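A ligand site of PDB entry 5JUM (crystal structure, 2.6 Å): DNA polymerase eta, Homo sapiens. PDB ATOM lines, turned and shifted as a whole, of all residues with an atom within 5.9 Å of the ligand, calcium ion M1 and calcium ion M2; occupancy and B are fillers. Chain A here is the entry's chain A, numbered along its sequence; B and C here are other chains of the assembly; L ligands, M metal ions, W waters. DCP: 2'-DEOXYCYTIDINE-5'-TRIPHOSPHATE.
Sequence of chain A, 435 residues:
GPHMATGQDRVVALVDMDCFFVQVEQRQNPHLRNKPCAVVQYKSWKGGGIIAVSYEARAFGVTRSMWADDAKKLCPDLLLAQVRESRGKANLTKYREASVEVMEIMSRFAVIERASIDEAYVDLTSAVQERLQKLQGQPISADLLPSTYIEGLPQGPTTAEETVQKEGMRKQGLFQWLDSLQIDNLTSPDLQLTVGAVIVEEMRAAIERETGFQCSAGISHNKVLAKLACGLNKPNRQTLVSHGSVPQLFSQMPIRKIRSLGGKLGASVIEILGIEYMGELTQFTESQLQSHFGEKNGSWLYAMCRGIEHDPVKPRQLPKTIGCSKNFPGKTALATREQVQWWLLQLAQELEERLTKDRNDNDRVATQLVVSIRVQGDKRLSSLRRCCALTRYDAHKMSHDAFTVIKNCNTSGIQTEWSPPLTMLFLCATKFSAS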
ATOM      1  N   ASP A  16      24.296 -19.498  12.557  1.00  0.00           N
ATOM      2  CA  ASP A  16      24.558 -18.084  12.653  1.00  0.00           C
ATOM      3  C   ASP A  16      25.962 -17.859  13.185  1.00  0.00           C
ATOM      4  O   ASP A  16      26.332 -18.470  14.195  1.00  0.00           O
ATOM      5  CB  ASP A  16      23.529 -17.423  13.557  1.00  0.00           C
ATOM      6  CG  ASP A  16      23.869 -16.000  13.830  1.00  0.00           C
ATOM      7  OD1 ASP A  16      23.491 -15.152  13.011  1.00  0.00           O
ATOM      8  OD2 ASP A  16      24.542 -15.737  14.835  1.00  0.00           O
ATOM      9  N   MET A  17      26.733 -17.007  12.527  1.00  0.00           N
ATOM     10  CA  MET A  17      28.141 -16.847  12.901  1.00  0.00           C
ATOM     11  C   MET A  17      28.269 -15.951  14.125  1.00  0.00           C
ATOM     12  O   MET A  17      27.572 -14.947  14.270  1.00  0.00           O
ATOM     13  CB  MET A  17      28.949 -16.272  11.736  1.00  0.00           C
ATOM     14  CG  MET A  17      28.637 -16.899  10.409  1.00  0.00           C
ATOM     15  SD  MET A  17      29.132 -18.620  10.343  1.00  0.00           S
ATOM     16  CE  MET A  17      30.809 -18.416  10.792  1.00  0.00           C
ATOM     17  N   ASP A  18      29.140 -16.343  15.031  1.00  0.00           N
ATOM     18  CA  ASP A  18      29.337 -15.539  16.225  1.00  0.00           C
ATOM     19  C   ASP A  18      30.050 -14.258  15.852  1.00  0.00           C
ATOM     20  O   ASP A  18      31.059 -14.295  15.154  1.00  0.00           O
ATOM     21  CB  ASP A  18      30.127 -16.338  17.256  1.00  0.00           C
ATOM     22  CG  ASP A  18      29.439 -17.637  17.623  1.00  0.00           C
ATOM     23  OD1 ASP A  18      28.194 -17.724  17.509  1.00  0.00           O
ATOM     24  OD2 ASP A  18      30.144 -18.573  18.042  1.00  0.00           O
ATOM     25  N   CYS A  19      29.505 -13.117  16.284  1.00  0.00           N
ATOM     26  CA  CYS A  19      30.075 -11.779  16.054  1.00  0.00           C
ATOM     27  C   CYS A  19      30.798 -11.685  14.707  1.00  0.00           C
ATOM     28  O   CYS A  19      32.012 -11.449  14.658  1.00  0.00           O
ATOM     29  CB  CYS A  19      31.002 -11.386  17.217  1.00  0.00           C
ATOM     30  SG  CYS A  19      32.363 -12.547  17.729  1.00  0.00           S
ATOM     31  N   PHE A  20      30.055 -11.870  13.619  1.00  0.00           N
ATOM     32  CA  PHE A  20      30.658 -12.243  12.340  1.00  0.00           C
ATOM     33  C   PHE A  20      31.761 -11.282  11.887  1.00  0.00           C
ATOM     34  O   PHE A  20      32.900 -11.698  11.644  1.00  0.00           O
ATOM     35  CB  PHE A  20      29.564 -12.339  11.291  1.00  0.00           C
ATOM     36  CG  PHE A  20      30.069 -12.819   9.971  1.00  0.00           C
ATOM     37  CD1 PHE A  20      30.847 -13.961   9.892  1.00  0.00           C
ATOM     38  CD2 PHE A  20      29.802 -12.108   8.817  1.00  0.00           C
ATOM     39  CE1 PHE A  20      31.343 -14.401   8.676  1.00  0.00           C
ATOM     40  CE2 PHE A  20      30.294 -12.543   7.589  1.00  0.00           C
ATOM     41  CZ  PHE A  20      31.054 -13.686   7.523  1.00  0.00           C
ATOM     42  N   PHE A  21      31.453  -9.983  11.739  1.00  0.00           N
ATOM     43  CA  PHE A  21      32.471  -9.040  11.259  1.00  0.00           C
ATOM     44  C   PHE A  21      33.699  -9.016  12.162  1.00  0.00           C
ATOM     45  O   PHE A  21      34.815  -8.809  11.662  1.00  0.00           O
ATOM     46  CB  PHE A  21      31.910  -7.637  11.133  1.00  0.00           C
ATOM     47  CG  PHE A  21      30.897  -7.458  10.050  1.00  0.00           C
ATOM     48  CD1 PHE A  21      30.177  -8.528   9.546  1.00  0.00           C
ATOM     49  CD2 PHE A  21      30.658  -6.197   9.538  1.00  0.00           C
ATOM     50  CE1 PHE A  21      29.223  -8.355   8.537  1.00  0.00           C
ATOM     51  CE2 PHE A  21      29.726  -6.010   8.543  1.00  0.00           C
ATOM     52  CZ  PHE A  21      29.001  -7.105   8.039  1.00  0.00           C
ATOM     53  N   VAL A  22      33.524  -9.222  13.473  1.00  0.00           N
ATOM     54  CA  VAL A  22      34.670  -9.249  14.375  1.00  0.00           C
ATOM     55  C   VAL A  22      35.555 -10.458  14.073  1.00  0.00           C
ATOM     56  O   VAL A  22      36.775 -10.337  13.910  1.00  0.00           O
ATOM     57  CB  VAL A  22      34.202  -9.205  15.844  1.00  0.00           C
ATOM     58  CG1 VAL A  22      35.346  -9.376  16.811  1.00  0.00           C
ATOM     59  CG2 VAL A  22      33.507  -7.877  16.139  1.00  0.00           C
ATOM     60  N   GLN A  41      32.352   1.892  11.496  1.00  0.00           N
ATOM     61  CA  GLN A  41      32.239   2.558  10.216  1.00  0.00           C
ATOM     62  C   GLN A  41      32.587   4.036  10.397  1.00  0.00           C
ATOM     63  O   GLN A  41      32.006   4.691  11.271  1.00  0.00           O
ATOM     64  CB  GLN A  41      30.835   2.415   9.636  1.00  0.00           C
ATOM     65  CG  GLN A  41      30.473   1.036   9.159  1.00  0.00           C
ATOM     66  CD  GLN A  41      29.054   0.983   8.617  1.00  0.00           C
ATOM     67  OE1 GLN A  41      28.751   0.165   7.749  1.00  0.00           O
ATOM     68  NE2 GLN A  41      28.183   1.848   9.117  1.00  0.00           N
ATOM     69  N   ILE A  51      29.377  -1.477  14.793  1.00  0.00           N
ATOM     70  CA  ILE A  51      28.384  -2.390  14.234  1.00  0.00           C
ATOM     71  C   ILE A  51      28.600  -3.848  14.650  1.00  0.00           C
ATOM     72  O   ILE A  51      27.712  -4.682  14.386  1.00  0.00           O
ATOM     73  CB  ILE A  51      28.285  -2.295  12.692  1.00  0.00           C
ATOM     74  CG1 ILE A  51      29.555  -2.778  11.993  1.00  0.00           C
ATOM     75  CG2 ILE A  51      27.969  -0.865  12.266  1.00  0.00           C
ATOM     76  CD1 ILE A  51      29.485  -2.550  10.498  1.00  0.00           C
ATOM     77  N   ALA A  52      29.725  -4.189  15.277  1.00  0.00           N
ATOM     78  CA  ALA A  52      29.914  -5.567  15.715  1.00  0.00           C
ATOM     79  C   ALA A  52      30.903  -5.583  16.880  1.00  0.00           C
ATOM     80  O   ALA A  52      31.835  -4.785  16.914  1.00  0.00           O
ATOM     81  CB  ALA A  52      30.382  -6.441  14.543  1.00  0.00           C
ATOM     82  N   VAL A  53      30.669  -6.484  17.827  1.00  0.00           N
ATOM     83  CA  VAL A  53      31.342  -6.475  19.122  1.00  0.00           C
ATOM     84  C   VAL A  53      31.755  -7.890  19.478  1.00  0.00           C
ATOM     85  O   VAL A  53      30.923  -8.811  19.423  1.00  0.00           O
ATOM     86  CB  VAL A  53      30.419  -5.897  20.230  1.00  0.00           C
ATOM     87  CG1 VAL A  53      31.166  -5.755  21.535  1.00  0.00           C
ATOM     88  CG2 VAL A  53      29.856  -4.555  19.823  1.00  0.00           C
ATOM     89  N   TYR A  55      32.673 -10.909  22.136  1.00  0.00           N
ATOM     90  CA  TYR A  55      32.044 -11.212  23.424  1.00  0.00           C
ATOM     91  C   TYR A  55      32.846 -10.708  24.628  1.00  0.00           C
ATOM     92  O   TYR A  55      32.254 -10.406  25.673  1.00  0.00           O
ATOM     93  CB  TYR A  55      31.773 -12.718  23.524  1.00  0.00           C
ATOM     94  CG  TYR A  55      30.606 -13.088  22.693  1.00  0.00           C
ATOM     95  CD1 TYR A  55      30.706 -13.185  21.317  1.00  0.00           C
ATOM     96  CD2 TYR A  55      29.368 -13.297  23.261  1.00  0.00           C
ATOM     97  CE1 TYR A  55      29.634 -13.514  20.536  1.00  0.00           C
ATOM     98  CE2 TYR A  55      28.267 -13.634  22.486  1.00  0.00           C
ATOM     99  CZ  TYR A  55      28.403 -13.737  21.120  1.00  0.00           C
ATOM    100  OH  TYR A  55      27.287 -14.054  20.348  1.00  0.00           O
ATOM    101  N   ARG A  58      31.650  -7.259  24.996  1.00  0.00           N
ATOM    102  CA  ARG A  58      30.287  -7.276  25.501  1.00  0.00           C
ATOM    103  C   ARG A  58      30.248  -7.380  27.027  1.00  0.00           C
ATOM    104  O   ARG A  58      29.353  -6.808  27.661  1.00  0.00           O
ATOM    105  CB  ARG A  58      29.508  -8.433  24.865  1.00  0.00           C
ATOM    106  CG  ARG A  58      29.303  -8.251  23.372  1.00  0.00           C
ATOM    107  CD  ARG A  58      28.325  -9.223  22.716  1.00  0.00           C
ATOM    108  NE  ARG A  58      28.693  -9.397  21.316  1.00  0.00           N
ATOM    109  CZ  ARG A  58      28.003 -10.063  20.395  1.00  0.00           C
ATOM    110  NH1 ARG A  58      26.850 -10.659  20.700  1.00  0.00           N
ATOM    111  NH2 ARG A  58      28.498 -10.150  19.153  1.00  0.00           N
ATOM    112  N   ARG A  64      26.396  -2.597  19.754  1.00  0.00           N
ATOM    113  CA  ARG A  64      26.236  -2.031  18.435  1.00  0.00           C
ATOM    114  C   ARG A  64      25.586  -0.663  18.543  1.00  0.00           C
ATOM    115  O   ARG A  64      25.036  -0.282  19.581  1.00  0.00           O
ATOM    116  CB  ARG A  64      25.408  -2.983  17.569  1.00  0.00           C
ATOM    117  CG  ARG A  64      25.319  -2.614  16.101  1.00  0.00           C
ATOM    118  CD  ARG A  64      24.277  -3.434  15.372  1.00  0.00           C
ATOM    119  NE  ARG A  64      24.838  -4.715  14.947  1.00  0.00           N
ATOM    120  CZ  ARG A  64      24.665  -5.854  15.599  1.00  0.00           C
ATOM    121  NH1 ARG A  64      23.924  -5.877  16.695  1.00  0.00           N
ATOM    122  NH2 ARG A  64      25.220  -6.964  15.153  1.00  0.00           N
ATOM    123  N   SER A  65      25.646   0.093  17.447  1.00  0.00           N
ATOM    124  CA  SER A  65      24.913   1.357  17.291  1.00  0.00           C
ATOM    125  C   SER A  65      25.229   2.292  18.457  1.00  0.00           C
ATOM    126  O   SER A  65      24.356   2.803  19.171  1.00  0.00           O
ATOM    127  CB  SER A  65      23.422   1.090  17.139  1.00  0.00           C
ATOM    128  OG  SER A  65      23.202   0.365  15.935  1.00  0.00           O
ATOM    129  N   SER A 116      20.575 -14.029   5.974  1.00  0.00           N
ATOM    130  CA  SER A 116      21.287 -12.782   6.201  1.00  0.00           C
ATOM    131  C   SER A 116      22.722 -12.994   5.715  1.00  0.00           C
ATOM    132  O   SER A 116      23.067 -14.050   5.189  1.00  0.00           O
ATOM    133  CB  SER A 116      21.192 -12.383   7.672  1.00  0.00           C
ATOM    134  OG  SER A 116      22.301 -12.853   8.414  1.00  0.00           O
ATOM    135  N   ILE A 117      23.568 -11.979   5.902  1.00  0.00           N
ATOM    136  CA  ILE A 117      24.955 -12.090   5.507  1.00  0.00           C
ATOM    137  C   ILE A 117      25.701 -13.162   6.303  1.00  0.00           C
ATOM    138  O   ILE A 117      26.734 -13.669   5.847  1.00  0.00           O
ATOM    139  CB  ILE A 117      25.666 -10.740   5.655  1.00  0.00           C
ATOM    140  CG1 ILE A 117      26.964 -10.727   4.839  1.00  0.00           C
ATOM    141  CG2 ILE A 117      25.919 -10.428   7.120  1.00  0.00           C
ATOM    142  CD1 ILE A 117      27.745  -9.444   4.988  1.00  0.00           C
ATOM    143  N   ASP A 118      25.187 -13.549   7.486  1.00  0.00           N
ATOM    144  CA  ASP A 118      25.883 -14.499   8.341  1.00  0.00           C
ATOM    145  C   ASP A 118      24.984 -15.595   8.902  1.00  0.00           C
ATOM    146  O   ASP A 118      25.391 -16.293   9.837  1.00  0.00           O
ATOM    147  CB  ASP A 118      26.585 -13.766   9.495  1.00  0.00           C
ATOM    148  CG  ASP A 118      25.655 -13.509  10.682  1.00  0.00           C
ATOM    149  OD1 ASP A 118      26.142 -13.588  11.837  1.00  0.00           O
ATOM    150  OD2 ASP A 118      24.450 -13.219  10.460  1.00  0.00           O
ATOM    151  N   GLU A 119      23.771 -15.771   8.384  1.00  0.00           N
ATOM    152  CA  GLU A 119      22.962 -16.889   8.846  1.00  0.00           C
ATOM    153  C   GLU A 119      22.182 -17.508   7.704  1.00  0.00           C
ATOM    154  O   GLU A 119      21.726 -16.805   6.793  1.00  0.00           O
ATOM    155  CB  GLU A 119      22.021 -16.494   9.994  1.00  0.00           C
ATOM    156  CG  GLU A 119      21.010 -15.447   9.654  1.00  0.00           C
ATOM    157  CD  GLU A 119      20.185 -15.064  10.840  1.00  0.00           C
ATOM    158  OE1 GLU A 119      18.954 -15.149  10.746  1.00  0.00           O
ATOM    159  OE2 GLU A 119      20.762 -14.684  11.878  1.00  0.00           O
ATOM    160  N   LYS A 227      15.497 -20.685  14.990  1.00  0.00           N
ATOM    161  CA  LYS A 227      16.082 -19.361  15.206  1.00  0.00           C
ATOM    162  C   LYS A 227      16.113 -19.022  16.702  1.00  0.00           C
ATOM    163  O   LYS A 227      17.126 -18.548  17.226  1.00  0.00           O
ATOM    164  CB  LYS A 227      15.292 -18.327  14.410  1.00  0.00           C
ATOM    165  CG  LYS A 227      15.686 -16.881  14.666  1.00  0.00           C
ATOM    166  CD  LYS A 227      17.147 -16.647  14.384  1.00  0.00           C
ATOM    167  CE  LYS A 227      17.557 -15.176  14.551  1.00  0.00           C
ATOM    168  NZ  LYS A 227      19.047 -14.995  14.444  1.00  0.00           N
ATOM    169  N   LYS A 234      24.575 -19.326  22.462  1.00  0.00           N
ATOM    170  CA  LYS A 234      25.686 -18.542  21.934  1.00  0.00           C
ATOM    171  C   LYS A 234      26.651 -18.210  23.055  1.00  0.00           C
ATOM    172  O   LYS A 234      26.238 -17.902  24.157  1.00  0.00           O
ATOM    173  CB  LYS A 234      25.179 -17.242  21.298  1.00  0.00           C
ATOM    174  CG  LYS A 234      24.658 -17.359  19.893  1.00  0.00           C
ATOM    175  CD  LYS A 234      24.293 -15.984  19.320  1.00  0.00           C
ATOM    176  CE  LYS A 234      24.136 -16.060  17.795  1.00  0.00           C
ATOM    177  NZ  LYS A 234      25.423 -16.372  17.083  1.00  0.00           N
ATOM    178  O5' 4E9 B   4      25.236   7.435  10.489  1.00  0.00           O
ATOM    179  C5' 4E9 B   4      25.851   6.398  11.204  1.00  0.00           C
ATOM    180  C4' 4E9 B   4      26.411   5.471  10.157  1.00  0.00           C
ATOM    181  O4' 4E9 B   4      26.404   4.198  10.787  1.00  0.00           O
ATOM    182  C1' 4E9 B   4      25.453   3.400  10.117  1.00  0.00           C
ATOM    183  N9  4E9 B   4      24.575   2.544  10.963  1.00  0.00           N
ATOM    184  C4  4E9 B   4      24.548   1.227  10.799  1.00  0.00           C
ATOM    185  N3  4E9 B   4      25.232   0.389   9.998  1.00  0.00           N
ATOM    186  C2  4E9 B   4      25.002  -0.938  10.057  1.00  0.00           C
ATOM    187  N1  4E9 B   4      24.111  -1.489  10.910  1.00  0.00           N
ATOM    188  C6  4E9 B   4      23.381  -0.757  11.765  1.00  0.00           C
ATOM    189  C5  4E9 B   4      23.561   0.691  11.766  1.00  0.00           C
ATOM    190  N7  4E9 B   4      23.055   1.724  12.451  1.00  0.00           N
ATOM    191  C8  4E9 B   4      23.688   2.799  11.948  1.00  0.00           C
ATOM    192  C2' 4E9 B   4      24.577   4.291   9.239  1.00  0.00           C
ATOM    193  C3' 4E9 B   4      25.518   5.420   8.914  1.00  0.00           C
ATOM    194  O3' 4E9 B   4      26.325   5.082   7.797  1.00  0.00           O
ATOM    195  P   4E9 B   4      23.741   7.941  10.749  1.00  0.00           P
ATOM    196  OP1 4E9 B   4      23.452   8.855   9.583  1.00  0.00           O
ATOM    197  OP2 4E9 B   4      22.833   6.748  10.704  1.00  0.00           O
ATOM    198  O6  4E9 B   4      22.565  -1.240  12.557  1.00  0.00           O
ATOM    199  N24 4E9 B   4      25.727  -1.698   9.194  1.00  0.00           N
ATOM    200  N8  4E9 B   4      23.426   4.047  12.403  1.00  0.00           N
ATOM    201  C10 4E9 B   4      22.999   4.338  13.668  1.00  0.00           C
ATOM    202  C11 4E9 B   4      23.861   4.787  14.692  1.00  0.00           C
ATOM    203  C12 4E9 B   4      25.232   4.950  14.450  1.00  0.00           C
ATOM    204  C13 4E9 B   4      26.084   5.393  15.467  1.00  0.00           C
ATOM    205  C14 4E9 B   4      25.572   5.691  16.737  1.00  0.00           C
ATOM    206  C15 4E9 B   4      24.209   5.547  16.991  1.00  0.00           C
ATOM    207  C16 4E9 B   4      23.717   5.854  18.266  1.00  0.00           C
ATOM    208  O27 4E9 B   4      24.512   6.247  19.156  1.00  0.00           O
ATOM    209  C17 4E9 B   4      22.352   5.719  18.571  1.00  0.00           C
ATOM    210  C18 4E9 B   4      21.860   6.022  19.837  1.00  0.00           C
ATOM    211  C19 4E9 B   4      20.512   5.884  20.120  1.00  0.00           C
ATOM    212  C20 4E9 B   4      19.638   5.437  19.141  1.00  0.00           C
ATOM    213  C21 4E9 B   4      20.124   5.123  17.880  1.00  0.00           C
ATOM    214  C22 4E9 B   4      21.478   5.273  17.592  1.00  0.00           C
ATOM    215  C23 4E9 B   4      22.001   4.942  16.236  1.00  0.00           C
ATOM    216  C24 4E9 B   4      21.144   4.493  15.234  1.00  0.00           C
ATOM    217  C26 4E9 B   4      23.360   5.091  15.969  1.00  0.00           C
ATOM    218  C25 4E9 B   4      21.643   4.201  13.962  1.00  0.00           C
ATOM    219  P    DA B   5      25.713   4.951   6.297  1.00  0.00           P
ATOM    220  OP1  DA B   5      26.720   5.476   5.367  1.00  0.00           O
ATOM    221  OP2  DA B   5      24.351   5.467   6.253  1.00  0.00           O
ATOM    222  O5'  DA B   5      25.605   3.375   6.039  1.00  0.00           O
ATOM    223  C5'  DA B   5      26.784   2.545   6.187  1.00  0.00           C
ATOM    224  C4'  DA B   5      26.596   1.161   5.585  1.00  0.00           C
ATOM    225  O4'  DA B   5      25.778   0.332   6.446  1.00  0.00           O
ATOM    226  C3'  DA B   5      25.922   1.101   4.224  1.00  0.00           C
ATOM    227  O3'  DA B   5      26.421  -0.022   3.547  1.00  0.00           O
ATOM    228  C2'  DA B   5      24.456   0.931   4.609  1.00  0.00           C
ATOM    229  C1'  DA B   5      24.591  -0.034   5.780  1.00  0.00           C
ATOM    230  N9   DA B   5      23.497   0.064   6.747  1.00  0.00           N
ATOM    231  C8   DA B   5      22.938   1.196   7.249  1.00  0.00           C
ATOM    232  N7   DA B   5      21.987   0.984   8.121  1.00  0.00           N
ATOM    233  C5   DA B   5      21.912  -0.387   8.218  1.00  0.00           C
ATOM    234  C6   DA B   5      21.100  -1.248   8.972  1.00  0.00           C
ATOM    235  N6   DA B   5      20.166  -0.812   9.803  1.00  0.00           N
ATOM    236  N1   DA B   5      21.256  -2.560   8.832  1.00  0.00           N
ATOM    237  C2   DA B   5      22.215  -3.009   8.004  1.00  0.00           C
ATOM    238  N3   DA B   5      23.046  -2.322   7.227  1.00  0.00           N
ATOM    239  C4   DA B   5      22.845  -0.985   7.382  1.00  0.00           C
ATOM    240  P    DT C   8      17.548 -10.473  13.820  1.00  0.00           P
ATOM    241  OP1  DT C   8      17.790 -11.779  14.495  1.00  0.00           O
ATOM    242  OP2  DT C   8      17.512  -9.209  14.564  1.00  0.00           O
ATOM    243  O5'  DT C   8      18.663 -10.261  12.679  1.00  0.00           O
ATOM    244  C5'  DT C   8      18.769 -11.127  11.550  1.00  0.00           C
ATOM    245  C4'  DT C   8      19.964 -10.731  10.704  1.00  0.00           C
ATOM    246  O4'  DT C   8      19.721  -9.437  10.111  1.00  0.00           O
ATOM    247  C3'  DT C   8      21.272 -10.603  11.464  1.00  0.00           C
ATOM    248  O3'  DT C   8      22.353 -11.090  10.664  1.00  0.00           O
ATOM    249  C2'  DT C   8      21.378  -9.113  11.708  1.00  0.00           C
ATOM    250  C1'  DT C   8      20.767  -8.560  10.428  1.00  0.00           C
ATOM    251  N1   DT C   8      20.203  -7.174  10.619  1.00  0.00           N
ATOM    252  C2   DT C   8      20.652  -6.128   9.817  1.00  0.00           C
ATOM    253  O2   DT C   8      21.476  -6.267   8.917  1.00  0.00           O
ATOM    254  N3   DT C   8      20.090  -4.919  10.098  1.00  0.00           N
ATOM    255  C4   DT C   8      19.164  -4.649  11.069  1.00  0.00           C
ATOM    256  O4   DT C   8      18.725  -3.522  11.243  1.00  0.00           O
ATOM    257  C5   DT C   8      18.746  -5.771  11.880  1.00  0.00           C
ATOM    258  C7   DT C   8      17.736  -5.571  12.968  1.00  0.00           C
ATOM    259  C6   DT C   8      19.288  -6.968  11.617  1.00  0.00           C
HETATM  260  N1  DCP L   1      25.190  -6.113  11.116  1.00  0.00           N
HETATM  261  C2  DCP L   1      25.159  -4.708  10.860  1.00  0.00           C
HETATM  262  N3  DCP L   1      24.154  -3.956  11.390  1.00  0.00           N
HETATM  263  C4  DCP L   1      23.220  -4.537  12.151  1.00  0.00           C
HETATM  264  C5  DCP L   1      23.253  -5.905  12.412  1.00  0.00           C
HETATM  265  C6  DCP L   1      24.254  -6.682  11.882  1.00  0.00           C
HETATM  266  O2  DCP L   1      26.064  -4.188  10.140  1.00  0.00           O
HETATM  267  N4  DCP L   1      22.217  -3.822  12.698  1.00  0.00           N
HETATM  268  C1' DCP L   1      26.273  -6.934  10.576  1.00  0.00           C
HETATM  269  C2' DCP L   1      27.421  -6.960  11.587  1.00  0.00           C
HETATM  270  C3' DCP L   1      27.336  -8.340  12.217  1.00  0.00           C
HETATM  271  C4' DCP L   1      26.660  -9.188  11.146  1.00  0.00           C
HETATM  272  O4' DCP L   1      25.814  -8.297  10.409  1.00  0.00           O
HETATM  273  O3' DCP L   1      28.616  -8.837  12.591  1.00  0.00           O
HETATM  274  C5' DCP L   1      25.781 -10.275  11.712  1.00  0.00           C
HETATM  275  O5' DCP L   1      24.845  -9.656  12.603  1.00  0.00           O
HETATM  276  PA  DCP L   1      24.285 -10.377  13.920  1.00  0.00           P
HETATM  277  O1A DCP L   1      24.265 -11.874  13.726  1.00  0.00           O
HETATM  278  O2A DCP L   1      22.936  -9.773  14.187  1.00  0.00           O
HETATM  279  O3A DCP L   1      25.221 -10.171  15.200  1.00  0.00           O
HETATM  280  PB  DCP L   1      26.754 -10.668  15.229  1.00  0.00           P
HETATM  281  O1B DCP L   1      26.978 -11.721  14.184  1.00  0.00           O
HETATM  282  O2B DCP L   1      27.662  -9.482  15.068  1.00  0.00           O
HETATM  283  O3B DCP L   1      27.080 -11.304  16.651  1.00  0.00           O
HETATM  284  PG  DCP L   1      26.158 -12.394  17.354  1.00  0.00           P
HETATM  285  O1G DCP L   1      25.329 -13.036  16.304  1.00  0.00           O
HETATM  286  O2G DCP L   1      25.314 -11.620  18.322  1.00  0.00           O
HETATM  287  O3G DCP L   1      27.092 -13.344  18.043  1.00  0.00           O
HETATM  288 CA    CA M   1      25.694 -13.701  14.057  1.00  0.00          CA
HETATM  289 CA    CA M   2      22.404 -13.036  12.549  1.00  0.00          CA
HETATM  290  O   HOH W   1      28.171  -7.848  17.233  1.00  0.00           O
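Four residues have an atom within 4 Å of calcium ion M2: Asp 16, Asp 118, Glu 119 and DT 8 of chain C.
Calcium ion M2 is bound by the side-chain carboxylate of Glu 119 (2.4 Å), the side-chain carboxylate of Asp 16 (2.4 Å), an oxygen (O1A) of the ligand (2.5 Å) and O3' of DT 8 of chain C (2.7 Å).
Calcium ion M2 has four donor atoms within binding distance.
Slightly farther from calcium ion M2 lies the side-chain carboxylate (OD2) of Asp 118 (2.9 Å).
OH of Tyr 55 sits at hydrogen-bond distance from NH1 of Arg 58, at 3.4 Å.
OE1 of Glu 119 is in salt-bridge range of NZ of Lys 227 (3.7 Å).
The side-chain carboxylate (OD2) of Asp 16 sits close to the side-chain amino group (NZ) of Lys 234 (2.5 Å).
O4' of 4E9 4 of chain B lies close to the side-chain amide nitrogen of Gln 41.
The side-chain amino group of Lys 227 is in salt-bridge range of OP1 of DT 8 of chain C (3.5 Å).
The guanidinium group of Arg 58 lies within hydrogen-bond range of the backbone carbonyl oxygen of Val 53 (2.8 Å).
The guanidinium group (NE) of Arg 64 lies within hydrogen-bond range of the backbone carbonyl oxygen (O) of Ile 51.
The side-chain amino group of Lys 234 is in salt-bridge range of the side-chain carboxylate of Asp 18 (3.1 Å).
Calcium ion M1 is bound by O of Met 17 (2.3 Å), OD1 of Asp 118 (2.3 Å), O1A of the ligand (2.3 Å), O1B of the ligand (2.4 Å), O1G of the ligand (2.4 Å), OD2 of Asp 16 (2.5 Å) and OD1 of Asp 16 (2.8 Å).
The side-chain hydroxyl (OH) of Tyr 55 lies within hydrogen-bond range of an oxygen (O3G) of the ligand (2.4 Å).
O6 of 4E9 4 of chain B sits at hydrogen-bond distance from N4 of the ligand (2.6 Å).
The guanidinium group of Arg 58 lies within salt-bridge range of an oxygen (O2G) of the ligand (3.0 Å).
N of Cys 19 lies within hydrogen-bond range of O3G of the ligand (3.0 Å).
The backbone NH (N) of Phe 20 sits close to an oxygen (O1B) of the ligand, 3.1 Å away.
The backbone NH of Phe 21 is in hydrogen-bond range of an oxygen (O3') of the ligand.
NH2 of Arg 64 is in salt-bridge range of O2B of the ligand (3.5 Å).
An oxygen (O3G) of the ligand lies within salt-bridge range of the side-chain amino group (NZ) of Lys 234 (3.6 Å).
Water W1 lies within hydrogen-bond range of O2B of the ligand, N of Val 53 and NH2 of Arg 58.
CA of Asp 18 touches O3G of the ligand, 3.6 Å away.
Ile 51 touches the ligand.
CB of Ala 52 touches O3' of the ligand (3.6 Å).
Ile 117 touches the ligand (CG2 to O4', 3.9 Å).
Hydrophobic or aromatic side chains within 4 Å of the ligand: Phe 20, Phe 21, Ile 51, Ala 52, Tyr 55 and Ile 117.
16 residues have an atom within 4 Å of the ligand: Asp 16, Met 17, Asp 18, Cys 19, Phe 20, Phe 21, Ile 51, Ala 52, Tyr 55, Arg 58, Arg 64, Ile 117, Asp 118, Lys 234, 4E9 4 of chain B and DT 8 of chain C.
Three residues have an atom within 4 Å of calcium ion M1: Asp 16, Met 17 and Asp 118.
The nearest printed residue that does not touch calcium ion M1 is Lys 234 (4.05 Å).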
